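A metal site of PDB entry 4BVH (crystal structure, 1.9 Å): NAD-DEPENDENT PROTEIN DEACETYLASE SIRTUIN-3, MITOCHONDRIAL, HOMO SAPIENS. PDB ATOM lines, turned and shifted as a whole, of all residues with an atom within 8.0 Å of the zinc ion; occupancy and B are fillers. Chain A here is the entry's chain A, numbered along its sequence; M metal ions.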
ATOM      1  N   THR A 140     -26.356  -6.947  13.332  1.00  0.00           N
ATOM      2  CA  THR A 140     -27.303  -6.644  14.407  1.00  0.00           C
ATOM      3  C   THR A 140     -28.221  -7.784  14.882  1.00  0.00           C
ATOM      4  O   THR A 140     -29.077  -8.280  14.118  1.00  0.00           O
ATOM      5  CB  THR A 140     -28.168  -5.453  13.987  1.00  0.00           C
ATOM      6  OG1 THR A 140     -27.313  -4.319  13.911  1.00  0.00           O
ATOM      7  CG2 THR A 140     -29.333  -5.194  14.988  1.00  0.00           C
ATOM      8  N   CYS A 141     -28.084  -8.133  16.167  1.00  0.00           N
ATOM      9  CA  CYS A 141     -29.014  -9.099  16.788  1.00  0.00           C
ATOM     10  C   CYS A 141     -30.479  -8.713  16.557  1.00  0.00           C
ATOM     11  O   CYS A 141     -30.899  -7.593  16.807  1.00  0.00           O
ATOM     12  CB  CYS A 141     -28.751  -9.313  18.287  1.00  0.00           C
ATOM     13  SG  CYS A 141     -29.673 -10.750  18.858  1.00  0.00           S
ATOM     14  N   THR A 142     -31.235  -9.671  16.017  1.00  0.00           N
ATOM     15  CA  THR A 142     -32.662  -9.561  15.734  1.00  0.00           C
ATOM     16  C   THR A 142     -33.509  -9.744  17.010  1.00  0.00           C
ATOM     17  O   THR A 142     -34.707  -9.503  16.991  1.00  0.00           O
ATOM     18  CB  THR A 142     -33.051 -10.693  14.813  1.00  0.00           C
ATOM     19  OG1 THR A 142     -32.463 -11.900  15.324  1.00  0.00           O
ATOM     20  CG2 THR A 142     -32.545 -10.433  13.345  1.00  0.00           C
ATOM     21  N   VAL A 143     -32.892 -10.209  18.095  1.00  0.00           N
ATOM     22  CA  VAL A 143     -33.594 -10.315  19.397  1.00  0.00           C
ATOM     23  C   VAL A 143     -33.235  -9.091  20.256  1.00  0.00           C
ATOM     24  O   VAL A 143     -34.086  -8.234  20.461  1.00  0.00           O
ATOM     25  CB  VAL A 143     -33.311 -11.668  20.102  1.00  0.00           C
ATOM     26  CG1 VAL A 143     -34.056 -11.757  21.440  1.00  0.00           C
ATOM     27  CG2 VAL A 143     -33.679 -12.816  19.164  1.00  0.00           C
ATOM     28  N   CYS A 144     -31.978  -8.983  20.687  1.00  0.00           N
ATOM     29  CA  CYS A 144     -31.577  -7.890  21.596  1.00  0.00           C
ATOM     30  C   CYS A 144     -31.090  -6.557  20.998  1.00  0.00           C
ATOM     31  O   CYS A 144     -30.990  -5.581  21.737  1.00  0.00           O
ATOM     32  CB  CYS A 144     -30.535  -8.391  22.555  1.00  0.00           C
ATOM     33  SG  CYS A 144     -28.965  -8.753  21.755  1.00  0.00           S
ATOM     34  N   GLN A 145     -30.775  -6.516  19.691  1.00  0.00           N
ATOM     35  CA  GLN A 145     -30.317  -5.285  18.985  1.00  0.00           C
ATOM     36  C   GLN A 145     -28.858  -4.909  19.214  1.00  0.00           C
ATOM     37  O   GLN A 145     -28.406  -3.855  18.756  1.00  0.00           O
ATOM     38  CB  GLN A 145     -31.203  -4.057  19.285  1.00  0.00           C
ATOM     39  CG  GLN A 145     -32.201  -3.699  18.219  1.00  0.00           C
ATOM     40  CD  GLN A 145     -33.301  -4.722  18.092  1.00  0.00           C
ATOM     41  OE1 GLN A 145     -33.449  -5.571  18.961  1.00  0.00           O
ATOM     42  NE2 GLN A 145     -34.068  -4.661  17.004  1.00  0.00           N
ATOM     43  N   ARG A 146     -28.118  -5.766  19.901  1.00  0.00           N
ATOM     44  CA  ARG A 146     -26.689  -5.517  20.095  1.00  0.00           C
ATOM     45  C   ARG A 146     -25.979  -5.472  18.714  1.00  0.00           C
ATOM     46  O   ARG A 146     -26.206  -6.355  17.893  1.00  0.00           O
ATOM     47  CB  ARG A 146     -26.045  -6.557  21.027  1.00  0.00           C
ATOM     48  CG  ARG A 146     -26.393  -6.368  22.515  1.00  0.00           C
ATOM     49  CD  ARG A 146     -25.673  -7.364  23.425  1.00  0.00           C
ATOM     50  NE  ARG A 146     -26.067  -7.247  24.827  1.00  0.00           N
ATOM     51  CZ  ARG A 146     -25.553  -6.377  25.704  1.00  0.00           C
ATOM     52  NH1 ARG A 146     -24.607  -5.507  25.349  1.00  0.00           N
ATOM     53  NH2 ARG A 146     -25.990  -6.366  26.954  1.00  0.00           N
ATOM     54  N   PRO A 147     -25.173  -4.419  18.467  1.00  0.00           N
ATOM     55  CA  PRO A 147     -24.425  -4.341  17.205  1.00  0.00           C
ATOM     56  C   PRO A 147     -23.168  -5.198  17.249  1.00  0.00           C
ATOM     57  O   PRO A 147     -22.594  -5.389  18.330  1.00  0.00           O
ATOM     58  CB  PRO A 147     -24.029  -2.874  17.129  1.00  0.00           C
ATOM     59  CG  PRO A 147     -23.964  -2.444  18.566  1.00  0.00           C
ATOM     60  CD  PRO A 147     -25.105  -3.164  19.222  1.00  0.00           C
ATOM     61  N   PHE A 148     -22.717  -5.686  16.097  1.00  0.00           N
ATOM     62  CA  PHE A 148     -21.522  -6.548  16.082  1.00  0.00           C
ATOM     63  C   PHE A 148     -20.487  -6.200  15.009  1.00  0.00           C
ATOM     64  O   PHE A 148     -20.831  -5.576  13.971  1.00  0.00           O
ATOM     65  CB  PHE A 148     -21.927  -8.034  15.964  1.00  0.00           C
ATOM     66  CG  PHE A 148     -22.701  -8.533  17.155  1.00  0.00           C
ATOM     67  CD1 PHE A 148     -24.084  -8.338  17.247  1.00  0.00           C
ATOM     68  CD2 PHE A 148     -22.043  -9.184  18.195  1.00  0.00           C
ATOM     69  CE1 PHE A 148     -24.790  -8.791  18.350  1.00  0.00           C
ATOM     70  CE2 PHE A 148     -22.737  -9.636  19.306  1.00  0.00           C
ATOM     71  CZ  PHE A 148     -24.118  -9.428  19.380  1.00  0.00           C
ATOM     72  N   ARG A 164     -25.330 -16.482  15.655  1.00  0.00           N
ATOM     73  CA  ARG A 164     -26.150 -16.287  16.852  1.00  0.00           C
ATOM     74  C   ARG A 164     -25.439 -15.337  17.829  1.00  0.00           C
ATOM     75  O   ARG A 164     -24.192 -15.303  17.935  1.00  0.00           O
ATOM     76  CB  ARG A 164     -26.500 -17.624  17.489  1.00  0.00           C
ATOM     77  CG  ARG A 164     -27.315 -18.513  16.570  1.00  0.00           C
ATOM     78  CD  ARG A 164     -28.170 -19.516  17.343  1.00  0.00           C
ATOM     79  NE  ARG A 164     -29.275 -20.003  16.519  1.00  0.00           N
ATOM     80  CZ  ARG A 164     -30.499 -19.456  16.503  1.00  0.00           C
ATOM     81  NH1 ARG A 164     -30.789 -18.406  17.246  1.00  0.00           N
ATOM     82  NH2 ARG A 164     -31.448 -19.961  15.714  1.00  0.00           N
ATOM     83  N   CYS A 165     -26.233 -14.534  18.503  1.00  0.00           N
ATOM     84  CA  CYS A 165     -25.699 -13.556  19.435  1.00  0.00           C
ATOM     85  C   CYS A 165     -24.892 -14.261  20.555  1.00  0.00           C
ATOM     86  O   CYS A 165     -25.390 -15.217  21.160  1.00  0.00           O
ATOM     87  CB  CYS A 165     -26.875 -12.804  19.990  1.00  0.00           C
ATOM     88  SG  CYS A 165     -26.477 -11.466  21.123  1.00  0.00           S
ATOM     89  N   PRO A 166     -23.624 -13.842  20.799  1.00  0.00           N
ATOM     90  CA  PRO A 166     -22.900 -14.408  21.959  1.00  0.00           C
ATOM     91  C   PRO A 166     -23.557 -14.072  23.298  1.00  0.00           C
ATOM     92  O   PRO A 166     -23.148 -14.613  24.326  1.00  0.00           O
ATOM     93  CB  PRO A 166     -21.529 -13.734  21.883  1.00  0.00           C
ATOM     94  CG  PRO A 166     -21.369 -13.314  20.465  1.00  0.00           C
ATOM     95  CD  PRO A 166     -22.754 -12.983  19.975  1.00  0.00           C
ATOM     96  N   VAL A 167     -24.561 -13.198  23.278  1.00  0.00           N
ATOM     97  CA  VAL A 167     -25.277 -12.787  24.500  1.00  0.00           C
ATOM     98  C   VAL A 167     -26.643 -13.492  24.666  1.00  0.00           C
ATOM     99  O   VAL A 167     -26.830 -14.227  25.628  1.00  0.00           O
ATOM    100  CB  VAL A 167     -25.418 -11.248  24.603  1.00  0.00           C
ATOM    101  CG1 VAL A 167     -26.273 -10.847  25.805  1.00  0.00           C
ATOM    102  CG2 VAL A 167     -24.051 -10.588  24.639  1.00  0.00           C
ATOM    103  N   CYS A 168     -27.582 -13.263  23.738  1.00  0.00           N
ATOM    104  CA  CYS A 168     -28.934 -13.842  23.887  1.00  0.00           C
ATOM    105  C   CYS A 168     -29.190 -15.132  23.049  1.00  0.00           C
ATOM    106  O   CYS A 168     -30.283 -15.705  23.109  1.00  0.00           O
ATOM    107  CB  CYS A 168     -30.043 -12.783  23.632  1.00  0.00           C
ATOM    108  SG  CYS A 168     -30.435 -12.366  21.892  1.00  0.00           S
ATOM    109  N   THR A 169     -28.162 -15.566  22.303  1.00  0.00           N
ATOM    110  CA  THR A 169     -28.261 -16.584  21.202  1.00  0.00           C
ATOM    111  C   THR A 169     -29.299 -16.350  20.034  1.00  0.00           C
ATOM    112  O   THR A 169     -29.481 -17.237  19.158  1.00  0.00           O
ATOM    113  CB  THR A 169     -28.343 -18.045  21.732  1.00  0.00           C
ATOM    114  OG1 THR A 169     -29.590 -18.233  22.424  1.00  0.00           O
ATOM    115  CG2 THR A 169     -27.120 -18.411  22.622  1.00  0.00           C
ATOM    116  N   GLY A 170     -29.944 -15.180  20.011  1.00  0.00           N
ATOM    117  CA  GLY A 170     -30.854 -14.795  18.921  1.00  0.00           C
ATOM    118  C   GLY A 170     -30.046 -14.687  17.626  1.00  0.00           C
ATOM    119  O   GLY A 170     -28.806 -14.560  17.649  1.00  0.00           O
ATOM    120  N   VAL A 171     -30.730 -14.819  16.496  1.00  0.00           N
ATOM    121  CA  VAL A 171     -30.063 -14.717  15.172  1.00  0.00           C
ATOM    122  C   VAL A 171     -29.482 -13.283  14.948  1.00  0.00           C
ATOM    123  O   VAL A 171     -30.178 -12.295  15.164  1.00  0.00           O
ATOM    124  CB  VAL A 171     -31.047 -15.108  14.039  1.00  0.00           C
ATOM    125  CG1 VAL A 171     -30.421 -14.852  12.674  1.00  0.00           C
ATOM    126  CG2 VAL A 171     -31.418 -16.587  14.170  1.00  0.00           C
ATOM    127  N   VAL A 172     -28.195 -13.199  14.590  1.00  0.00           N
ATOM    128  CA  VAL A 172     -27.580 -11.906  14.192  1.00  0.00           C
ATOM    129  C   VAL A 172     -27.732 -11.782  12.641  1.00  0.00           C
ATOM    130  O   VAL A 172     -27.348 -12.700  11.900  1.00  0.00           O
ATOM    131  CB  VAL A 172     -26.064 -11.809  14.537  1.00  0.00           C
ATOM    132  CG1 VAL A 172     -25.563 -10.388  14.268  1.00  0.00           C
ATOM    133  CG2 VAL A 172     -25.740 -12.239  15.992  1.00  0.00           C
HETATM  134 ZN    ZN M   1     -28.625 -10.885  21.104  1.00  0.00          ZN
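The backbone carbonyl oxygen (O) of Gly 170 is in hydrogen-bond range of the backbone NH (N) of Cys 165, 2.7 Å away. SG of Cys 165 lies close to N of Val 167 (3.4 Å). The side-chain sulfur (SG) of Cys 144 lies close to the backbone NH (N) of Arg 146 (3.6 Å). SG of Cys 168 lies close to N of Gly 170. SG of Cys 141 sits close to N of Val 143, at 3.4 Å. The backbone carbonyl oxygen of Arg 146 sits at hydrogen-bond distance from the backbone NH of Cys 141.
Four residues have an atom within 4 Å of the zinc ion: Cys 141, Cys 144, Cys 165 and Cys 168. Along chain A the residues within 4 Å of the zinc ion span positions 141 to 168. The nearest printed residue that does not touch the zinc ion is Gly 170 (4.6 Å).
The zinc ion is bound by SG of Cys 165 (2.2 Å), SG of Cys 144 (2.3 Å), SG of Cys 168 (2.5 Å) and SG of Cys 141 (2.5 Å). The zinc ion has four donor atoms within binding distance.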
